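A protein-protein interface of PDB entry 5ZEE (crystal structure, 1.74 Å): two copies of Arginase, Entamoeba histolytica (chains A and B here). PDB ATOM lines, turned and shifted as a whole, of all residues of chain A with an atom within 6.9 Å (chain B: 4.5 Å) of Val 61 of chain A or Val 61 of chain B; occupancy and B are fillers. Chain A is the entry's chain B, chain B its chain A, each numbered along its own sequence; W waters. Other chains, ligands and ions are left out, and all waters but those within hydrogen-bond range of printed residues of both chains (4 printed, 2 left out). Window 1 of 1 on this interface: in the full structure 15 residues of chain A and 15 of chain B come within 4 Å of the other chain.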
ATOM      1  N   GLU A  20      -1.454   1.942  -5.997  1.00  0.00           N
ATOM      2  CA  GLU A  20      -2.893   1.704  -6.002  1.00  0.00           C
ATOM      3  C   GLU A  20      -3.210   0.327  -5.418  1.00  0.00           C
ATOM      4  O   GLU A  20      -4.145   0.181  -4.656  1.00  0.00           O
ATOM      5  CB  GLU A  20      -3.475   1.801  -7.403  1.00  0.00           C
ATOM      6  CG  GLU A  20      -3.577   3.209  -7.929  1.00  0.00           C
ATOM      7  CD  GLU A  20      -4.614   4.047  -7.176  1.00  0.00           C
ATOM      8  OE1 GLU A  20      -5.667   3.515  -6.712  1.00  0.00           O
ATOM      9  OE2 GLU A  20      -4.368   5.252  -7.022  1.00  0.00           O
ATOM     10  N   LYS A  21      -2.416  -0.650  -5.751  1.00  0.00           N
ATOM     11  CA  LYS A  21      -2.640  -2.003  -5.241  1.00  0.00           C
ATOM     12  C   LYS A  21      -1.388  -2.818  -5.159  1.00  0.00           C
ATOM     13  O   LYS A  21      -0.441  -2.568  -5.860  1.00  0.00           O
ATOM     14  CB  LYS A  21      -3.697  -2.736  -6.085  1.00  0.00           C
ATOM     15  CG  LYS A  21      -3.215  -3.079  -7.475  1.00  0.00           C
ATOM     16  CD  LYS A  21      -4.189  -4.054  -8.158  1.00  0.00           C
ATOM     17  CE  LYS A  21      -3.888  -4.341  -9.618  1.00  0.00           C
ATOM     18  NZ  LYS A  21      -2.443  -4.475  -9.914  1.00  0.00           N
ATOM     19  N   VAL A  22      -1.372  -3.785  -4.254  1.00  0.00           N
ATOM     20  CA  VAL A  22      -0.360  -4.818  -4.271  1.00  0.00           C
ATOM     21  C   VAL A  22      -1.084  -6.110  -4.597  1.00  0.00           C
ATOM     22  O   VAL A  22      -2.123  -6.378  -4.021  1.00  0.00           O
ATOM     23  CB  VAL A  22       0.329  -4.982  -2.905  1.00  0.00           C
ATOM     24  CG1 VAL A  22       1.251  -6.185  -2.914  1.00  0.00           C
ATOM     25  CG2 VAL A  22       1.125  -3.720  -2.569  1.00  0.00           C
ATOM     26  N   THR A  23      -0.513  -6.919  -5.474  1.00  0.00           N
ATOM     27  CA  THR A  23      -0.992  -8.274  -5.652  1.00  0.00           C
ATOM     28  C   THR A  23      -0.108  -9.201  -4.820  1.00  0.00           C
ATOM     29  O   THR A  23       1.108  -9.204  -5.000  1.00  0.00           O
ATOM     30  CB  THR A  23      -0.960  -8.681  -7.110  1.00  0.00           C
ATOM     31  OG1 THR A  23      -1.774  -7.782  -7.882  1.00  0.00           O
ATOM     32  CG2 THR A  23      -1.517 -10.139  -7.261  1.00  0.00           C
ATOM     33  N   TYR A  24      -0.742  -9.975  -3.936  1.00  0.00           N
ATOM     34  CA  TYR A  24      -0.028 -10.897  -3.061  1.00  0.00           C
ATOM     35  C   TYR A  24      -0.448 -12.322  -3.412  1.00  0.00           C
ATOM     36  O   TYR A  24      -1.613 -12.668  -3.236  1.00  0.00           O
ATOM     37  CB  TYR A  24      -0.313 -10.525  -1.606  1.00  0.00           C
ATOM     38  CG  TYR A  24      -0.079 -11.596  -0.544  1.00  0.00           C
ATOM     39  CD1 TYR A  24       0.918 -12.558  -0.676  1.00  0.00           C
ATOM     40  CD2 TYR A  24      -0.909 -11.682   0.568  1.00  0.00           C
ATOM     41  CE1 TYR A  24       1.086 -13.568   0.278  1.00  0.00           C
ATOM     42  CE2 TYR A  24      -0.734 -12.689   1.525  1.00  0.00           C
ATOM     43  CZ  TYR A  24       0.251 -13.640   1.359  1.00  0.00           C
ATOM     44  OH  TYR A  24       0.422 -14.644   2.305  1.00  0.00           O
ATOM     45  N   PHE A  50       2.535  -9.651   8.094  1.00  0.00           N
ATOM     46  CA  PHE A  50       2.768  -9.362   6.668  1.00  0.00           C
ATOM     47  C   PHE A  50       1.683  -8.451   6.060  1.00  0.00           C
ATOM     48  O   PHE A  50       2.023  -7.485   5.349  1.00  0.00           O
ATOM     49  CB  PHE A  50       2.889 -10.661   5.887  1.00  0.00           C
ATOM     50  CG  PHE A  50       3.080 -10.479   4.407  1.00  0.00           C
ATOM     51  CD1 PHE A  50       4.188  -9.847   3.907  1.00  0.00           C
ATOM     52  CD2 PHE A  50       2.145 -10.952   3.517  1.00  0.00           C
ATOM     53  CE1 PHE A  50       4.341  -9.646   2.542  1.00  0.00           C
ATOM     54  CE2 PHE A  50       2.300 -10.779   2.161  1.00  0.00           C
ATOM     55  CZ  PHE A  50       3.414 -10.145   1.660  1.00  0.00           C
ATOM     56  N   MET A  51       0.424  -8.702   6.381  1.00  0.00           N
ATOM     57  CA  MET A  51      -0.664  -7.868   5.809  1.00  0.00           C
ATOM     58  C   MET A  51      -0.567  -6.423   6.307  1.00  0.00           C
ATOM     59  O   MET A  51      -0.901  -5.504   5.593  1.00  0.00           O
ATOM     60  CB  MET A  51      -2.036  -8.418   6.126  1.00  0.00           C
ATOM     61  CG  MET A  51      -2.262  -9.839   5.611  1.00  0.00           C
ATOM     62  SD  MET A  51      -2.231  -9.958   3.817  1.00  0.00           S
ATOM     63  CE  MET A  51      -3.663  -8.956   3.343  1.00  0.00           C
ATOM     64  N   LEU A  54       1.982  -4.670   4.205  1.00  0.00           N
ATOM     65  CA  LEU A  54       1.375  -4.288   2.922  1.00  0.00           C
ATOM     66  C   LEU A  54       0.439  -3.081   3.040  1.00  0.00           C
ATOM     67  O   LEU A  54       0.299  -2.305   2.098  1.00  0.00           O
ATOM     68  CB  LEU A  54       0.606  -5.478   2.302  1.00  0.00           C
ATOM     69  CG  LEU A  54       1.396  -6.692   1.918  1.00  0.00           C
ATOM     70  CD1 LEU A  54       0.506  -7.733   1.235  1.00  0.00           C
ATOM     71  CD2 LEU A  54       2.537  -6.280   1.028  1.00  0.00           C
ATOM     72  N   GLU A  55      -0.214  -2.932   4.185  1.00  0.00           N
ATOM     73  CA  GLU A  55      -1.089  -1.802   4.475  1.00  0.00           C
ATOM     74  C   GLU A  55      -0.352  -0.435   4.444  1.00  0.00           C
ATOM     75  O   GLU A  55      -0.972   0.584   4.200  1.00  0.00           O
ATOM     76  CB  GLU A  55      -1.757  -1.976   5.846  1.00  0.00           C
ATOM     77  CG  GLU A  55      -3.256  -1.703   5.902  1.00  0.00           C
ATOM     78  CD  GLU A  55      -3.913  -2.054   7.233  1.00  0.00           C
ATOM     79  OE1 GLU A  55      -3.466  -1.483   8.247  1.00  0.00           O
ATOM     80  OE2 GLU A  55      -4.902  -2.868   7.261  1.00  0.00           O
ATOM     81  N   ALA A  58      -0.190   0.061   0.272  1.00  0.00           N
ATOM     82  CA  ALA A  58      -1.375   0.212  -0.603  1.00  0.00           C
ATOM     83  C   ALA A  58      -2.640   0.017   0.213  1.00  0.00           C
ATOM     84  O   ALA A  58      -2.677  -0.804   1.136  1.00  0.00           O
ATOM     85  CB  ALA A  58      -1.320  -0.805  -1.713  1.00  0.00           C
ATOM     86  N   LYS A  59      -3.679   0.729  -0.163  1.00  0.00           N
ATOM     87  CA  LYS A  59      -4.971   0.538   0.442  1.00  0.00           C
ATOM     88  C   LYS A  59      -5.700  -0.696  -0.090  1.00  0.00           C
ATOM     89  O   LYS A  59      -6.699  -1.080   0.507  1.00  0.00           O
ATOM     90  CB  LYS A  59      -5.861   1.760   0.235  1.00  0.00           C
ATOM     91  CG  LYS A  59      -5.423   2.952   1.060  1.00  0.00           C
ATOM     92  CD  LYS A  59      -6.090   4.226   0.550  1.00  0.00           C
ATOM     93  CE  LYS A  59      -7.617   4.234   0.716  1.00  0.00           C
ATOM     94  NZ  LYS A  59      -8.033   4.133   2.155  1.00  0.00           N
ATOM     95  N   SER A  60      -5.283  -1.224  -1.242  1.00  0.00           N
ATOM     96  CA  SER A  60      -5.903  -2.420  -1.835  1.00  0.00           C
ATOM     97  C   SER A  60      -4.868  -3.497  -1.935  1.00  0.00           C
ATOM     98  O   SER A  60      -3.777  -3.257  -2.470  1.00  0.00           O
ATOM     99  CB  SER A  60      -6.432  -2.134  -3.246  1.00  0.00           C
ATOM    100  OG  SER A  60      -7.607  -1.379  -3.169  1.00  0.00           O
ATOM    101  N   VAL A  61      -5.160  -4.689  -1.410  1.00  0.00           N
ATOM    102  CA  VAL A  61      -4.301  -5.842  -1.574  1.00  0.00           C
ATOM    103  C   VAL A  61      -5.183  -6.914  -2.185  1.00  0.00           C
ATOM    104  O   VAL A  61      -6.240  -7.236  -1.631  1.00  0.00           O
ATOM    105  CB  VAL A  61      -3.672  -6.361  -0.253  1.00  0.00           C
ATOM    106  CG1 VAL A  61      -2.916  -7.631  -0.494  1.00  0.00           C
ATOM    107  CG2 VAL A  61      -2.729  -5.318   0.335  1.00  0.00           C
ATOM    108  N   ASN A  62      -4.777  -7.409  -3.350  1.00  0.00           N
ATOM    109  CA  ASN A  62      -5.478  -8.505  -4.018  1.00  0.00           C
ATOM    110  C   ASN A  62      -4.671  -9.768  -3.729  1.00  0.00           C
ATOM    111  O   ASN A  62      -3.605  -9.981  -4.307  1.00  0.00           O
ATOM    112  CB  ASN A  62      -5.587  -8.247  -5.540  1.00  0.00           C
ATOM    113  CG  ASN A  62      -6.448  -7.025  -5.880  1.00  0.00           C
ATOM    114  OD1 ASN A  62      -6.385  -6.520  -7.010  1.00  0.00           O
ATOM    115  ND2 ASN A  62      -7.278  -6.569  -4.945  1.00  0.00           N
ATOM    116  N   LYS A  63      -5.178 -10.612  -2.849  1.00  0.00           N
ATOM    117  CA  LYS A  63      -4.474 -11.830  -2.500  1.00  0.00           C
ATOM    118  C   LYS A  63      -5.030 -12.954  -3.331  1.00  0.00           C
ATOM    119  O   LYS A  63      -6.263 -13.089  -3.446  1.00  0.00           O
ATOM    120  CB  LYS A  63      -4.627 -12.166  -1.022  1.00  0.00           C
ATOM    121  CG  LYS A  63      -3.917 -13.453  -0.655  1.00  0.00           C
ATOM    122  CD  LYS A  63      -4.029 -13.905   0.787  1.00  0.00           C
ATOM    123  CE  LYS A  63      -3.339 -15.274   0.953  1.00  0.00           C
ATOM    124  NZ  LYS A  63      -3.757 -15.843   2.260  1.00  0.00           N
ATOM    125  N   LYS A  64      -4.128 -13.786  -3.837  1.00  0.00           N
ATOM    126  CA  LYS A  64      -4.488 -15.050  -4.485  1.00  0.00           C
ATOM    127  C   LYS A  64      -3.738 -16.164  -3.763  1.00  0.00           C
ATOM    128  O   LYS A  64      -2.584 -15.978  -3.393  1.00  0.00           O
ATOM    129  CB  LYS A  64      -3.997 -15.051  -5.933  1.00  0.00           C
ATOM    130  CG  LYS A  64      -4.297 -13.803  -6.749  1.00  0.00           C
ATOM    131  CD  LYS A  64      -5.777 -13.661  -6.994  1.00  0.00           C
ATOM    132  CE  LYS A  64      -6.039 -12.417  -7.850  1.00  0.00           C
ATOM    133  NZ  LYS A  64      -7.479 -12.064  -7.815  1.00  0.00           N
ATOM    134  N   THR A  65      -4.338 -17.333  -3.640  1.00  0.00           N
ATOM    135  CA  THR A  65      -3.668 -18.493  -3.099  1.00  0.00           C
ATOM    136  C   THR A  65      -3.594 -19.565  -4.171  1.00  0.00           C
ATOM    137  O   THR A  65      -4.610 -19.981  -4.708  1.00  0.00           O
ATOM    138  CB  THR A  65      -4.413 -19.070  -1.881  1.00  0.00           C
ATOM    139  OG1 THR A  65      -4.599 -18.033  -0.904  1.00  0.00           O
ATOM    140  CG2 THR A  65      -3.608 -20.243  -1.222  1.00  0.00           C
ATOM    141  N   VAL B  22     -13.805 -13.177  -1.813  1.00  0.00           N
ATOM    142  CA  VAL B  22     -14.316 -12.504  -0.653  1.00  0.00           C
ATOM    143  C   VAL B  22     -13.729 -11.105  -0.703  1.00  0.00           C
ATOM    144  O   VAL B  22     -12.536 -10.953  -0.966  1.00  0.00           O
ATOM    145  CB  VAL B  22     -13.848 -13.179   0.647  1.00  0.00           C
ATOM    146  CG1 VAL B  22     -14.185 -12.301   1.860  1.00  0.00           C
ATOM    147  CG2 VAL B  22     -14.480 -14.559   0.781  1.00  0.00           C
ATOM    148  N   TYR B  24     -12.767  -8.154   1.719  1.00  0.00           N
ATOM    149  CA  TYR B  24     -12.458  -7.994   3.131  1.00  0.00           C
ATOM    150  C   TYR B  24     -12.087  -6.509   3.315  1.00  0.00           C
ATOM    151  O   TYR B  24     -11.097  -6.051   2.776  1.00  0.00           O
ATOM    152  CB  TYR B  24     -11.326  -8.946   3.527  1.00  0.00           C
ATOM    153  CG  TYR B  24     -10.521  -8.584   4.771  1.00  0.00           C
ATOM    154  CD1 TYR B  24     -11.103  -7.903   5.851  1.00  0.00           C
ATOM    155  CD2 TYR B  24      -9.141  -8.872   4.847  1.00  0.00           C
ATOM    156  CE1 TYR B  24     -10.349  -7.530   6.965  1.00  0.00           C
ATOM    157  CE2 TYR B  24      -8.389  -8.520   5.980  1.00  0.00           C
ATOM    158  CZ  TYR B  24      -9.001  -7.824   7.019  1.00  0.00           C
ATOM    159  OH  TYR B  24      -8.275  -7.429   8.137  1.00  0.00           O
ATOM    160  N   MET B  51      -6.694 -14.540   7.668  1.00  0.00           N
ATOM    161  CA  MET B  51      -6.490 -14.763   6.228  1.00  0.00           C
ATOM    162  C   MET B  51      -6.505 -16.255   5.902  1.00  0.00           C
ATOM    163  O   MET B  51      -6.947 -16.631   4.819  1.00  0.00           O
ATOM    164  CB  MET B  51      -5.186 -14.168   5.725  1.00  0.00           C
ATOM    165  CG  MET B  51      -5.060 -12.659   5.930  1.00  0.00           C
ATOM    166  SD  MET B  51      -6.306 -11.683   5.074  1.00  0.00           S
ATOM    167  CE  MET B  51      -5.859 -11.976   3.374  1.00  0.00           C
ATOM    168  N   LEU B  54     -10.105 -17.245   5.567  1.00  0.00           N
ATOM    169  CA  LEU B  54     -10.623 -16.825   4.260  1.00  0.00           C
ATOM    170  C   LEU B  54     -10.137 -17.690   3.105  1.00  0.00           C
ATOM    171  O   LEU B  54     -10.861 -17.862   2.113  1.00  0.00           O
ATOM    172  CB  LEU B  54     -10.262 -15.359   3.996  1.00  0.00           C
ATOM    173  CG  LEU B  54     -10.887 -14.301   4.898  1.00  0.00           C
ATOM    174  CD1 LEU B  54     -10.629 -12.893   4.361  1.00  0.00           C
ATOM    175  CD2 LEU B  54     -12.387 -14.514   4.991  1.00  0.00           C
ATOM    176  N   LYS B  59     -10.299 -18.545  -3.268  1.00  0.00           N
ATOM    177  CA  LYS B  59      -8.888 -18.376  -3.649  1.00  0.00           C
ATOM    178  C   LYS B  59      -8.503 -16.914  -3.838  1.00  0.00           C
ATOM    179  O   LYS B  59      -7.307 -16.614  -3.871  1.00  0.00           O
ATOM    180  CB  LYS B  59      -8.552 -19.114  -4.942  1.00  0.00           C
ATOM    181  CG  LYS B  59      -8.563 -20.618  -4.780  1.00  0.00           C
ATOM    182  CD  LYS B  59      -8.629 -21.283  -6.130  1.00  0.00           C
ATOM    183  CE  LYS B  59      -7.403 -21.047  -7.019  1.00  0.00           C
ATOM    184  NZ  LYS B  59      -6.185 -21.648  -6.403  1.00  0.00           N
ATOM    185  N   SER B  60      -9.489 -16.025  -3.992  1.00  0.00           N
ATOM    186  CA  SER B  60      -9.233 -14.595  -4.160  1.00  0.00           C
ATOM    187  C   SER B  60      -9.816 -13.848  -2.992  1.00  0.00           C
ATOM    188  O   SER B  60     -10.989 -14.044  -2.659  1.00  0.00           O
ATOM    189  CB  SER B  60      -9.878 -14.086  -5.434  1.00  0.00           C
ATOM    190  OG  SER B  60      -9.131 -14.481  -6.556  1.00  0.00           O
ATOM    191  N   VAL B  61      -8.989 -13.044  -2.323  1.00  0.00           N
ATOM    192  CA  VAL B  61      -9.460 -12.140  -1.298  1.00  0.00           C
ATOM    193  C   VAL B  61      -9.027 -10.750  -1.739  1.00  0.00           C
ATOM    194  O   VAL B  61      -7.843 -10.512  -1.955  1.00  0.00           O
ATOM    195  CB  VAL B  61      -8.875 -12.457   0.099  1.00  0.00           C
ATOM    196  CG1 VAL B  61      -9.286 -11.379   1.094  1.00  0.00           C
ATOM    197  CG2 VAL B  61      -9.309 -13.840   0.574  1.00  0.00           C
ATOM    198  N   ASN B  62      -9.991  -9.846  -1.909  1.00  0.00           N
ATOM    199  CA  ASN B  62      -9.734  -8.459  -2.229  1.00  0.00           C
ATOM    200  C   ASN B  62      -9.853  -7.689  -0.912  1.00  0.00           C
ATOM    201  O   ASN B  62     -10.950  -7.453  -0.425  1.00  0.00           O
ATOM    202  CB  ASN B  62     -10.733  -7.927  -3.270  1.00  0.00           C
ATOM    203  CG  ASN B  62     -10.574  -8.569  -4.631  1.00  0.00           C
ATOM    204  OD1 ASN B  62      -9.572  -9.222  -4.927  1.00  0.00           O
ATOM    205  ND2 ASN B  62     -11.554  -8.350  -5.487  1.00  0.00           N
ATOM    206  N   LYS B  63      -8.717  -7.270  -0.362  1.00  0.00           N
ATOM    207  CA  LYS B  63      -8.725  -6.550   0.842  1.00  0.00           C
ATOM    208  C   LYS B  63      -8.681  -5.060   0.537  1.00  0.00           C
ATOM    209  O   LYS B  63      -7.880  -4.625  -0.299  1.00  0.00           O
ATOM    210  CB  LYS B  63      -7.530  -6.885   1.737  1.00  0.00           C
ATOM    211  CG  LYS B  63      -7.526  -6.085   3.042  1.00  0.00           C
ATOM    212  CD  LYS B  63      -6.363  -6.340   3.954  1.00  0.00           C
ATOM    213  CE  LYS B  63      -6.414  -5.418   5.185  1.00  0.00           C
ATOM    214  NZ  LYS B  63      -5.110  -5.447   5.912  1.00  0.00           N
HETATM  215  O   HOH W   1      -8.367  -5.154  -3.009  1.00  0.00           O
HETATM  216  O   HOH W   2      -3.149  -5.206   4.097  1.00  0.00           O
HETATM  217  O   HOH W   3      -6.383 -15.577   2.390  1.00  0.00           O
HETATM  218  O   HOH W   4      -3.402  -4.810   8.801  1.00  0.00           O
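The backbone carbonyl oxygen (O) of Val 22 of chain B sits at hydrogen-bond distance from the backbone NH (N) of Asn 62 of chain B (2.9 Å).
The backbone NH of Asn 62 of chain A lies within hydrogen-bond range of the backbone carbonyl oxygen of Val 22 of chain A (2.9 Å).
N of Tyr 24 of chain B lies within hydrogen-bond range of O of Asn 62 of chain B, 2.9 Å away.
O of Tyr 24 of chain A lies within hydrogen-bond range of N of Lys 64 of chain A (2.8 Å).
N of Val 22 of chain A lies within hydrogen-bond range of O of Ser 60 of chain A, at 3.0 Å.
The backbone NH of Tyr 24 of chain A lies within hydrogen-bond range of the backbone carbonyl oxygen of Asn 62 of chain A (2.9 Å).
Among the printed residues, pairs that only touch across the chains: Lys 64 of chain A with Lys 59 of chain B (3.3 Å), Ser 60 of chain A with Lys 63 of chain B (3.3 Å), Lys 63 of chain A with Ser 60 of chain B (3.4 Å), Asn 62 of chain A with Asn 62 of chain B (3.5 Å), Val 61 of chain A with Val 61 of chain B (3.7 Å), Lys 63 of chain A with Lys 59 of chain B (3.7 Å), Asn 62 of chain A with Val 61 of chain B (3.7 Å), Lys 63 of chain A with Met 51 of chain B (3.7 Å), Val 61 of chain A with Asn 62 of chain B (3.7 Å), Met 51 of chain A with Met 51 of chain B (3.7 Å), Met 51 of chain A with Lys 63 of chain B (3.8 Å) and Lys 59 of chain A with Lys 63 of chain B (3.8 Å).
Water W1 lies within hydrogen-bond range of the side-chain amide nitrogen (ND2) of Asn 62 of chain A (2.6 Å), the backbone carbonyl oxygen (O) of Lys 63 of chain B (2.8 Å) and the backbone carbonyl oxygen (O) of Val 61 of chain A (3.3 Å).
Water W3 bridges NZ of Lys 63 of chain A (2.6 Å) and O of Met 51 of chain B (2.7 Å).
Water W2 lies within hydrogen-bond range of the side-chain amino group (NZ) of Lys 63 of chain B and the backbone carbonyl oxygen (O) of Met 51 of chain A.
Water W4 lies within hydrogen-bond range of the side-chain carboxylate of Glu 55 of chain A (2.9 Å) and the side-chain amino group of Lys 63 of chain B (3.4 Å).
Met 51 of chain A touches Lys 63 of chain B, and with the chains exchanged Lys 63 of chain A touches Met 51 of chain B.
Lys 59 of chain A touches Lys 63 of chain B, and with the chains exchanged Lys 63 of chain A touches Lys 59 of chain B.
Val 61 of chain A touches Asn 62 of chain B, and with the chains exchanged Asn 62 of chain A touches Val 61 of chain B.
Val 61 of chain A touches Lys 63 of chain B, and with the chains exchanged Lys 63 of chain A touches Val 61 of chain B.
9 positions are printed for both chains.
NZ of Lys 63 of chain B is in salt-bridge range of OE2 of Glu 55 of chain A (2.9 Å).
The backbone NH (N) of Lys 63 of chain B sits at hydrogen-bond distance from the backbone carbonyl oxygen (O) of Val 61 of chain A, 2.8 Å away.
NZ of Lys 59 of chain B is in hydrogen-bond range of O of Thr 65 of chain A (2.9 Å).
OG of Ser 60 of chain B lies within hydrogen-bond range of NZ of Lys 64 of chain A (3.2 Å).
The backbone carbonyl oxygen (O) of Val 61 of chain B sits at hydrogen-bond distance from the backbone NH (N) of Lys 63 of chain A (2.8 Å).
Hydrophobic or aromatic side chains of chain A within 4 Å of the printed part of chain B: Met 51.
Of the 9 printed residues of chain B, 6 touch a printed residue of chain A.
Hydrophobic or aromatic side chains of chain B within 4 Å of the printed part of chain A: Met 51.
Among the printed residues, 17 pairs touch across the chains.
Among the printed residues, Asp or Glu carboxylates within 4 Å of a Lys or Arg side-chain nitrogen of the other chain: Glu 55 of chain A with Lys 63 of chain B (2.9 Å).
Val 61 of chain A touches just these residues of chain B: Val 61 (3.7 Å), Asn 62 (3.7 Å) and Lys 63 (2.8 Å).
Of chain A, only Val 61 (3.7 Å), Asn 62 (3.7 Å) and Lys 63 (2.8 Å) come within 4 Å of Val 61 of chain B.
Printed residues of chain B within 4 Å of Ser 60 of chain A: Lys 63.
Printed residues of chain B within 4 Å of Glu 55 of chain A: Lys 63 (2.9 Å).
Of the printed residues of chain B, Lys 64 of chain A touches Lys 59 and Ser 60.
Printed residues of chain B within 4 Å of Lys 63 of chain A: Met 51 (3.7 Å), Lys 59 (3.7 Å), Ser 60 (3.4 Å) and Val 61 (2.8 Å).
Of the printed residues of chain A, Met 51 of chain B touches Met 51 and Lys 63.
Lys 21 of chain A touches none of the printed residues of chain B.
Val 22 of chain B touches none of the printed residues of chain A.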
